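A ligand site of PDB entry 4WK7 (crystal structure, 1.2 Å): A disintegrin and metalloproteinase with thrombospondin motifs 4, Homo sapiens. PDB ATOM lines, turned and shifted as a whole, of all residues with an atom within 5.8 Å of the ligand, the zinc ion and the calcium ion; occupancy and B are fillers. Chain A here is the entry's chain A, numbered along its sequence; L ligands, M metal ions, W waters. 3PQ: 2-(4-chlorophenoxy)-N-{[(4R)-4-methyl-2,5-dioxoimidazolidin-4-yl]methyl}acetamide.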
ATOM      1  N   GLN A 107      12.525  11.034 -26.649  1.00  0.00           N
ATOM      2  CA  GLN A 107      13.236   9.999 -27.401  1.00  0.00           C
ATOM      3  C   GLN A 107      14.214   9.258 -26.498  1.00  0.00           C
ATOM      4  O   GLN A 107      14.950   9.879 -25.731  1.00  0.00           O
ATOM      5  CB  GLN A 107      13.994  10.620 -28.583  1.00  0.00           C
ATOM      6  CG  GLN A 107      14.926   9.684 -29.347  1.00  0.00           C
ATOM      7  CD  GLN A 107      14.187   8.610 -30.130  1.00  0.00           C
ATOM      8  OE1 GLN A 107      13.274   8.909 -30.898  1.00  0.00           O
ATOM      9  NE2 GLN A 107      14.585   7.361 -29.933  1.00  0.00           N
ATOM     10  N   ASP A 108      14.208   7.931 -26.582  1.00  0.00           N
ATOM     11  CA  ASP A 108      15.195   7.103 -25.912  1.00  0.00           C
ATOM     12  C   ASP A 108      16.522   7.253 -26.643  1.00  0.00           C
ATOM     13  O   ASP A 108      16.693   6.718 -27.753  1.00  0.00           O
ATOM     14  CB  ASP A 108      14.743   5.635 -25.879  1.00  0.00           C
ATOM     15  CG  ASP A 108      15.671   4.738 -25.081  1.00  0.00           C
ATOM     16  OD1 ASP A 108      16.685   5.225 -24.521  1.00  0.00           O
ATOM     17  OD2 ASP A 108      15.400   3.520 -24.995  1.00  0.00           O
ATOM     18  N   LEU A 109      17.440   7.996 -26.047  1.00  0.00           N
ATOM     19  CA  LEU A 109      18.750   8.235 -26.644  1.00  0.00           C
ATOM     20  C   LEU A 109      19.672   7.055 -26.405  1.00  0.00           C
ATOM     21  O   LEU A 109      19.662   6.460 -25.320  1.00  0.00           O
ATOM     22  CB  LEU A 109      19.380   9.506 -26.059  1.00  0.00           C
ATOM     23  CG  LEU A 109      18.585  10.794 -26.286  1.00  0.00           C
ATOM     24  CD1 LEU A 109      19.239  11.946 -25.520  1.00  0.00           C
ATOM     25  CD2 LEU A 109      18.473  11.121 -27.769  1.00  0.00           C
ATOM     26  N   CYS A 110      20.471   6.721 -27.407  1.00  0.00           N
ATOM     27  CA  CYS A 110      21.311   5.540 -27.367  1.00  0.00           C
ATOM     28  C   CYS A 110      22.739   5.836 -27.810  1.00  0.00           C
ATOM     29  O   CYS A 110      22.995   6.810 -28.538  1.00  0.00           O
ATOM     30  CB  CYS A 110      20.730   4.428 -28.243  1.00  0.00           C
ATOM     31  SG  CYS A 110      18.950   4.120 -28.024  1.00  0.00           S
ATOM     32  N   CYS A 115      21.120   1.591 -24.990  1.00  0.00           N
ATOM     33  CA  CYS A 115      20.314   2.813 -24.889  1.00  0.00           C
ATOM     34  C   CYS A 115      20.273   3.343 -23.451  1.00  0.00           C
ATOM     35  O   CYS A 115      19.355   4.083 -23.091  1.00  0.00           O
ATOM     36  CB  CYS A 115      18.910   2.557 -25.424  1.00  0.00           C
ATOM     37  SG  CYS A 115      18.844   2.264 -27.203  1.00  0.00           S
ATOM     38  N   ASP A 116      21.270   2.979 -22.648  1.00  0.00           N
ATOM     39  CA  ASP A 116      21.323   3.404 -21.252  1.00  0.00           C
ATOM     40  C   ASP A 116      21.565   4.901 -21.088  1.00  0.00           C
ATOM     41  O   ASP A 116      21.204   5.492 -20.072  1.00  0.00           O
ATOM     42  CB  ASP A 116      22.414   2.637 -20.490  1.00  0.00           C
ATOM     43  CG  ASP A 116      22.191   1.137 -20.503  1.00  0.00           C
ATOM     44  OD1 ASP A 116      21.022   0.700 -20.604  1.00  0.00           O
ATOM     45  OD2 ASP A 116      23.190   0.397 -20.391  1.00  0.00           O
ATOM     46  N   THR A 117      22.186   5.516 -22.100  1.00  0.00           N
ATOM     47  CA  THR A 117      22.501   6.940 -22.026  1.00  0.00           C
ATOM     48  C   THR A 117      21.236   7.779 -21.881  1.00  0.00           C
ATOM     49  O   THR A 117      20.174   7.446 -22.406  1.00  0.00           O
ATOM     50  CB  THR A 117      23.356   7.433 -23.225  1.00  0.00           C
ATOM     51  OG1 THR A 117      23.774   8.785 -22.977  1.00  0.00           O
ATOM     52  CG2 THR A 117      22.582   7.377 -24.540  1.00  0.00           C
ATOM     53  N   LEU A 118      21.368   8.873 -21.131  1.00  0.00           N
ATOM     54  CA  LEU A 118      20.275   9.812 -20.913  1.00  0.00           C
ATOM     55  C   LEU A 118      20.563  11.201 -21.490  1.00  0.00           C
ATOM     56  O   LEU A 118      19.737  12.098 -21.369  1.00  0.00           O
ATOM     57  CB  LEU A 118      19.999   9.949 -19.411  1.00  0.00           C
ATOM     58  CG  LEU A 118      19.419   8.707 -18.729  1.00  0.00           C
ATOM     59  CD1 LEU A 118      19.425   8.902 -17.220  1.00  0.00           C
ATOM     60  CD2 LEU A 118      18.011   8.421 -19.230  1.00  0.00           C
ATOM     61  N   GLY A 119      21.714  11.384 -22.125  1.00  0.00           N
ATOM     62  CA  GLY A 119      22.037  12.695 -22.667  1.00  0.00           C
ATOM     63  C   GLY A 119      23.423  12.767 -23.236  1.00  0.00           C
ATOM     64  O   GLY A 119      24.203  11.816 -23.136  1.00  0.00           O
ATOM     65  N   MET A 120      23.730  13.897 -23.859  1.00  0.00           N
ATOM     66  CA  MET A 120      25.039  14.126 -24.483  1.00  0.00           C
ATOM     67  C   MET A 120      25.287  15.626 -24.615  1.00  0.00           C
ATOM     68  O   MET A 120      24.366  16.393 -24.834  1.00  0.00           O
ATOM     69  CB  MET A 120      25.091  13.445 -25.863  1.00  0.00           C
ATOM     70  CG  MET A 120      26.489  13.264 -26.449  1.00  0.00           C
ATOM     71  SD  MET A 120      26.573  12.431 -28.061  1.00  0.00           S
ATOM     72  CE  MET A 120      26.913  10.740 -27.585  1.00  0.00           C
ATOM     73  N   ALA A 121      26.559  16.019 -24.511  1.00  0.00           N
ATOM     74  CA  ALA A 121      26.944  17.396 -24.718  1.00  0.00           C
ATOM     75  C   ALA A 121      28.368  17.425 -25.227  1.00  0.00           C
ATOM     76  O   ALA A 121      29.117  16.487 -24.986  1.00  0.00           O
ATOM     77  CB  ALA A 121      26.854  18.174 -23.411  1.00  0.00           C
ATOM     78  N   GLU A 137      17.510  13.266 -22.417  1.00  0.00           N
ATOM     79  CA  GLU A 137      16.352  12.382 -22.446  1.00  0.00           C
ATOM     80  C   GLU A 137      15.553  12.621 -21.166  1.00  0.00           C
ATOM     81  O   GLU A 137      16.049  12.363 -20.079  1.00  0.00           O
ATOM     82  CB  GLU A 137      16.809  10.921 -22.505  1.00  0.00           C
ATOM     83  CG  GLU A 137      15.667   9.923 -22.438  1.00  0.00           C
ATOM     84  CD  GLU A 137      16.147   8.490 -22.494  1.00  0.00           C
ATOM     85  OE1 GLU A 137      17.176   8.215 -23.152  1.00  0.00           O
ATOM     86  OE2 GLU A 137      15.484   7.627 -21.876  1.00  0.00           O
ATOM     87  N   PHE A 145      18.988  16.491 -12.931  1.00  0.00           N
ATOM     88  CA  PHE A 145      20.315  15.930 -12.686  1.00  0.00           C
ATOM     89  C   PHE A 145      21.043  15.657 -14.002  1.00  0.00           C
ATOM     90  O   PHE A 145      22.218  15.977 -14.145  1.00  0.00           O
ATOM     91  CB  PHE A 145      20.241  14.671 -11.821  1.00  0.00           C
ATOM     92  CG  PHE A 145      19.965  14.959 -10.370  1.00  0.00           C
ATOM     93  CD1 PHE A 145      20.979  15.438  -9.541  1.00  0.00           C
ATOM     94  CD2 PHE A 145      18.704  14.761  -9.829  1.00  0.00           C
ATOM     95  CE1 PHE A 145      20.738  15.715  -8.208  1.00  0.00           C
ATOM     96  CE2 PHE A 145      18.459  15.023  -8.490  1.00  0.00           C
ATOM     97  CZ  PHE A 145      19.468  15.509  -7.679  1.00  0.00           C
ATOM     98  N   THR A 146      20.343  15.067 -14.973  1.00  0.00           N
ATOM     99  CA  THR A 146      20.941  14.861 -16.285  1.00  0.00           C
ATOM    100  C   THR A 146      21.299  16.199 -16.930  1.00  0.00           C
ATOM    101  O   THR A 146      22.389  16.350 -17.489  1.00  0.00           O
ATOM    102  CB  THR A 146      20.023  14.037 -17.199  1.00  0.00           C
ATOM    103  OG1 THR A 146      19.742  12.793 -16.541  1.00  0.00           O
ATOM    104  CG2 THR A 146      20.686  13.749 -18.544  1.00  0.00           C
ATOM    105  N   HIS A 149      24.435  17.394 -15.358  1.00  0.00           N
ATOM    106  CA  HIS A 149      25.570  16.612 -15.844  1.00  0.00           C
ATOM    107  C   HIS A 149      26.029  17.092 -17.220  1.00  0.00           C
ATOM    108  O   HIS A 149      27.221  17.314 -17.456  1.00  0.00           O
ATOM    109  CB  HIS A 149      25.190  15.118 -15.880  1.00  0.00           C
ATOM    110  CG  HIS A 149      26.281  14.220 -16.365  1.00  0.00           C
ATOM    111  ND1 HIS A 149      27.157  13.585 -15.520  1.00  0.00           N
ATOM    112  CD2 HIS A 149      26.638  13.842 -17.620  1.00  0.00           C
ATOM    113  CE1 HIS A 149      28.013  12.864 -16.225  1.00  0.00           C
ATOM    114  NE2 HIS A 149      27.717  13.003 -17.497  1.00  0.00           N
ATOM    115  N   GLU A 150      25.065  17.282 -18.118  1.00  0.00           N
ATOM    116  CA  GLU A 150      25.405  17.710 -19.475  1.00  0.00           C
ATOM    117  C   GLU A 150      25.962  19.130 -19.496  1.00  0.00           C
ATOM    118  O   GLU A 150      26.937  19.411 -20.189  1.00  0.00           O
ATOM    119  CB  GLU A 150      24.185  17.600 -20.410  1.00  0.00           C
ATOM    120  CG  GLU A 150      23.618  16.190 -20.530  1.00  0.00           C
ATOM    121  CD  GLU A 150      24.650  15.139 -20.876  1.00  0.00           C
ATOM    122  OE1 GLU A 150      25.659  15.460 -21.541  1.00  0.00           O
ATOM    123  OE2 GLU A 150      24.429  13.963 -20.505  1.00  0.00           O
ATOM    124  N   HIS A 153      29.514  19.110 -18.469  1.00  0.00           N
ATOM    125  CA  HIS A 153      30.374  18.884 -19.629  1.00  0.00           C
ATOM    126  C   HIS A 153      30.592  20.152 -20.459  1.00  0.00           C
ATOM    127  O   HIS A 153      31.713  20.458 -20.852  1.00  0.00           O
ATOM    128  CB  HIS A 153      29.806  17.805 -20.541  1.00  0.00           C
ATOM    129  CG  HIS A 153      29.984  16.402 -20.038  1.00  0.00           C
ATOM    130  ND1 HIS A 153      31.177  15.932 -19.539  1.00  0.00           N
ATOM    131  CD2 HIS A 153      29.119  15.361 -20.016  1.00  0.00           C
ATOM    132  CE1 HIS A 153      31.037  14.653 -19.217  1.00  0.00           C
ATOM    133  NE2 HIS A 153      29.796  14.289 -19.500  1.00  0.00           N
ATOM    134  N   HIS A 159      34.370  13.209 -16.254  1.00  0.00           N
ATOM    135  CA  HIS A 159      33.764  12.258 -15.341  1.00  0.00           C
ATOM    136  C   HIS A 159      34.641  12.032 -14.122  1.00  0.00           C
ATOM    137  O   HIS A 159      35.866  12.062 -14.210  1.00  0.00           O
ATOM    138  CB  HIS A 159      33.508  10.921 -16.013  1.00  0.00           C
ATOM    139  CG  HIS A 159      32.427  10.974 -17.041  1.00  0.00           C
ATOM    140  ND1 HIS A 159      32.437  10.187 -18.166  1.00  0.00           N
ATOM    141  CD2 HIS A 159      31.310  11.733 -17.116  1.00  0.00           C
ATOM    142  CE1 HIS A 159      31.364  10.443 -18.885  1.00  0.00           C
ATOM    143  NE2 HIS A 159      30.670  11.383 -18.281  1.00  0.00           N
ATOM    144  N   HIS A 177      28.432  12.124  -7.036  1.00  0.00           N
ATOM    145  CA  HIS A 177      28.424  13.497  -7.553  1.00  0.00           C
ATOM    146  C   HIS A 177      27.758  13.565  -8.921  1.00  0.00           C
ATOM    147  O   HIS A 177      27.535  12.544  -9.564  1.00  0.00           O
ATOM    148  CB  HIS A 177      29.852  14.036  -7.658  1.00  0.00           C
ATOM    149  CG  HIS A 177      30.659  13.871  -6.412  1.00  0.00           C
ATOM    150  ND1 HIS A 177      30.445  14.633  -5.274  1.00  0.00           N
ATOM    151  CD2 HIS A 177      31.690  13.048  -6.118  1.00  0.00           C
ATOM    152  CE1 HIS A 177      31.304  14.272  -4.343  1.00  0.00           C
ATOM    153  NE2 HIS A 177      32.073  13.311  -4.823  1.00  0.00           N
ATOM    154  N   VAL A 178      27.478  14.780  -9.354  1.00  0.00           N
ATOM    155  CA  VAL A 178      26.800  15.019 -10.635  1.00  0.00           C
ATOM    156  C   VAL A 178      27.597  14.471 -11.828  1.00  0.00           C
ATOM    157  O   VAL A 178      27.008  13.950 -12.763  1.00  0.00           O
ATOM    158  CB  VAL A 178      26.487  16.517 -10.826  1.00  0.00           C
ATOM    159  CG1 VAL A 178      26.008  16.813 -12.254  1.00  0.00           C
ATOM    160  CG2 VAL A 178      25.422  16.955  -9.826  1.00  0.00           C
ATOM    161  N   MET A 179      28.929  14.553 -11.760  1.00  0.00           N
ATOM    162  CA  MET A 179      29.757  14.111 -12.874  1.00  0.00           C
ATOM    163  C   MET A 179      30.232  12.662 -12.763  1.00  0.00           C
ATOM    164  O   MET A 179      31.185  12.265 -13.424  1.00  0.00           O
ATOM    165  CB  MET A 179      30.929  15.071 -13.079  1.00  0.00           C
ATOM    166  CG  MET A 179      30.504  16.500 -13.419  1.00  0.00           C
ATOM    167  SD  MET A 179      29.258  16.646 -14.739  1.00  0.00           S
ATOM    168  CE  MET A 179      30.139  15.914 -16.116  1.00  0.00           C
ATOM    169  N   ALA A 180      29.545  11.853 -11.945  1.00  0.00           N
ATOM    170  CA  ALA A 180      29.660  10.406 -12.074  1.00  0.00           C
ATOM    171  C   ALA A 180      29.256  10.036 -13.509  1.00  0.00           C
ATOM    172  O   ALA A 180      28.439  10.726 -14.113  1.00  0.00           O
ATOM    173  CB  ALA A 180      28.756   9.701 -11.071  1.00  0.00           C
ATOM    174  N   PRO A 181      29.842   8.967 -14.074  1.00  0.00           N
ATOM    175  CA  PRO A 181      29.531   8.606 -15.457  1.00  0.00           C
ATOM    176  C   PRO A 181      28.108   8.092 -15.673  1.00  0.00           C
ATOM    177  O   PRO A 181      27.581   8.182 -16.784  1.00  0.00           O
ATOM    178  CB  PRO A 181      30.558   7.520 -15.782  1.00  0.00           C
ATOM    179  CG  PRO A 181      30.923   6.945 -14.454  1.00  0.00           C
ATOM    180  CD  PRO A 181      30.846   8.078 -13.480  1.00  0.00           C
ATOM    181  N   VAL A 182      27.514   7.545 -14.619  1.00  0.00           N
ATOM    182  CA  VAL A 182      26.125   7.095 -14.649  1.00  0.00           C
ATOM    183  C   VAL A 182      25.413   7.684 -13.447  1.00  0.00           C
ATOM    184  O   VAL A 182      26.035   7.922 -12.413  1.00  0.00           O
ATOM    185  CB  VAL A 182      26.022   5.553 -14.630  1.00  0.00           C
ATOM    186  CG1 VAL A 182      26.714   4.953 -15.842  1.00  0.00           C
ATOM    187  CG2 VAL A 182      26.580   4.957 -13.342  1.00  0.00           C
ATOM    188  N   MET A 183      24.124   7.925 -13.587  1.00  0.00           N
ATOM    189  CA  MET A 183      23.355   8.521 -12.498  1.00  0.00           C
ATOM    190  C   MET A 183      23.344   7.612 -11.271  1.00  0.00           C
ATOM    191  O   MET A 183      23.016   6.431 -11.354  1.00  0.00           O
ATOM    192  CB  MET A 183      21.924   8.816 -12.932  1.00  0.00           C
ATOM    193  CG  MET A 183      21.181   9.683 -11.932  1.00  0.00           C
ATOM    194  SD  MET A 183      19.477  10.003 -12.398  1.00  0.00           S
ATOM    195  CE  MET A 183      19.688  11.011 -13.856  1.00  0.00           C
ATOM    196  N   ALA A 184      23.724   8.187 -10.140  1.00  0.00           N
ATOM    197  CA  ALA A 184      23.604   7.534  -8.838  1.00  0.00           C
ATOM    198  C   ALA A 184      23.111   8.594  -7.866  1.00  0.00           C
ATOM    199  O   ALA A 184      23.018   9.776  -8.228  1.00  0.00           O
ATOM    200  CB  ALA A 184      24.941   6.992  -8.395  1.00  0.00           C
ATOM    201  N   VAL A 186      22.999  11.460  -5.604  1.00  0.00           N
ATOM    202  CA  VAL A 186      23.929  12.587  -5.465  1.00  0.00           C
ATOM    203  C   VAL A 186      23.961  13.090  -4.030  1.00  0.00           C
ATOM    204  O   VAL A 186      22.925  13.276  -3.405  1.00  0.00           O
ATOM    205  CB  VAL A 186      23.538  13.732  -6.434  1.00  0.00           C
ATOM    206  CG1 VAL A 186      24.391  14.974  -6.199  1.00  0.00           C
ATOM    207  CG2 VAL A 186      23.683  13.268  -7.880  1.00  0.00           C
HETATM  208  C7  3PQ L   1      28.144   9.697 -20.230  1.00  0.00           C
HETATM  209  C6  3PQ L   1      27.359   8.454 -22.181  1.00  0.00           C
HETATM  210  N1  3PQ L   1      28.113  11.064 -20.152  1.00  0.00           N
HETATM  211  C5  3PQ L   1      26.918   9.277 -20.985  1.00  0.00           C
HETATM  212  C2  3PQ L   1      27.060  11.598 -20.819  1.00  0.00           C
HETATM  213  C16 3PQ L   1      23.301  11.750 -15.351  1.00  0.00           C
HETATM  214  C21 3PQ L   1      25.406  10.980 -14.539  1.00  0.00           C
HETATM  215  C17 3PQ L   1      23.039  12.309 -14.109  1.00  0.00           C
HETATM  216  C20 3PQ L   1      25.134  11.531 -13.309  1.00  0.00           C
HETATM  217  C13 3PQ L   1      23.860  10.625 -17.780  1.00  0.00           C
HETATM  218  C9  3PQ L   1      26.022   8.488 -20.042  1.00  0.00           C
HETATM  219  C15 3PQ L   1      24.490  11.087 -15.567  1.00  0.00           C
HETATM  220  C18 3PQ L   1      23.955  12.197 -13.095  1.00  0.00           C
HETATM  221  C11 3PQ L   1      24.335   9.919 -19.030  1.00  0.00           C
HETATM  222  N4  3PQ L   1      26.377  10.550 -21.373  1.00  0.00           N
HETATM  223  N10 3PQ L   1      25.559   9.293 -18.936  1.00  0.00           N
HETATM  224  O8  3PQ L   1      28.986   8.955 -19.759  1.00  0.00           O
HETATM  225  O3  3PQ L   1      26.810  12.800 -20.893  1.00  0.00           O
HETATM  226  O12 3PQ L   1      23.668   9.911 -20.043  1.00  0.00           O
HETATM  227  O14 3PQ L   1      24.859  10.490 -16.769  1.00  0.00           O
HETATM  228 CL1  3PQ L   1      23.633  12.888 -11.529  1.00  0.00          CL
HETATM  229 ZN    ZN M   1      29.013  12.404 -18.994  1.00  0.00          ZN
HETATM  230 CA    CA M   2      18.385   6.177 -23.344  1.00  0.00          CA
HETATM  231  O   HOH W   1      25.626   9.947 -24.648  1.00  0.00           O
HETATM  232  O   HOH W   2      17.259   5.536 -21.307  1.00  0.00           O
HETATM  233  O   HOH W   3      28.191   5.960 -18.630  1.00  0.00           O
HETATM  234  O   HOH W   4      23.396   6.824 -18.553  1.00  0.00           O
HETATM  235  O   HOH W   5      28.176  13.997 -23.065  1.00  0.00           O
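A nitrogen (N1) of the ligand binds the zinc ion (2.0 Å).
NE2 of His 149 is bound to the zinc ion, 2.1 Å away.
The zinc ion is bound by NE2 of His 159, at 2.1 Å.
The zinc ion is bound by NE2 of His 153 (2.1 Å).
The side-chain hydroxyl (OG1) of Thr 117 sits at hydrogen-bond distance from an oxygen (O12) of the ligand.
The side-chain carboxylate (OE2) of Glu 150 sits close to an oxygen (O3) of the ligand, at 2.7 Å.
The backbone NH (N) of Leu 118 is in hydrogen-bond range of an oxygen (O12) of the ligand (2.7 Å).
An oxygen (O12) of the ligand is in hydrogen-bond range of the backbone NH of Gly 119 (3.2 Å).
The backbone carbonyl oxygen (O) of Gly 119 lies within hydrogen-bond range of a nitrogen (N4) of the ligand, 3.1 Å away.
A nitrogen (N10) of the ligand lies within hydrogen-bond range of the backbone carbonyl oxygen (O) of Pro 181, 3.2 Å away.
OD1 of Asp 108 binds the calcium ion (2.3 Å).
The calcium ion is bound by O of Cys 115 (2.3 Å).
O of Leu 109 is bound to the calcium ion, 2.4 Å away.
OE1 of Glu 137 binds the calcium ion (2.4 Å).
The calcium ion is bound by O of Thr 117 (2.4 Å).
The calcium ion is bound by water W2 (2.4 Å).
Water W5 lies within hydrogen-bond range of O3 of the ligand (2.8 Å), N of Ala 121 (3.0 Å) and OE1 of Glu 150 (3.3 Å).
Water W4 bridges the backbone carbonyl oxygen of Asp 116 (3.0 Å) and a nitrogen (N10) of the ligand (3.3 Å).
Water W3 bridges O of Pro 181 and O8 of the ligand.
Water W1 lies within hydrogen-bond range of the side-chain hydroxyl of Thr 117 (2.8 Å), the backbone carbonyl oxygen of Gly 119 (2.8 Å) and a nitrogen (N4) of the ligand (3.4 Å).
The nearest printed residue that does not touch the calcium ion is Asp 116 (4.1 Å).
O of Ala 180 sits close to ND1 of His 149 (3.4 Å).
A ring nitrogen (ND1) of His 149 is in hydrogen-bond range of the backbone carbonyl oxygen (O) of Val 178.
ND1 of His 149 lies close to SD of Met 179 (3.8 Å).
The side-chain sulfur (SG) of Cys 115 forms a disulfide with the side-chain sulfur (SG) of Cys 110 (2.0 Å).
N of Glu 137 lies within hydrogen-bond range of O of Leu 118 (2.7 Å).
OG1 of Thr 117 sits at hydrogen-bond distance from O of Gly 119.
The backbone NH (N) of Met 120 lies close to the side-chain carboxylate (OE1) of Glu 150, at 3.4 Å.
OE1 of Glu 150 sits at hydrogen-bond distance from N of Ala 121 (3.2 Å).
Merely in contact with the ligand: Phe 145 (3.8 Å), Thr 146 (3.9 Å), Val 178 (3.1 Å), Ala 180 (3.1 Å), Val 182 (3.5 Å), Met 183 (3.4 Å) and Val 186 (3.7 Å).
Hydrophobic or aromatic side chains that line the ligand: Leu 118, Phe 145, His 149, His 153, His 159, Met 183 and Val 186.
Along chain A the residues within 4 Å of the ligand span positions 117 to 186.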
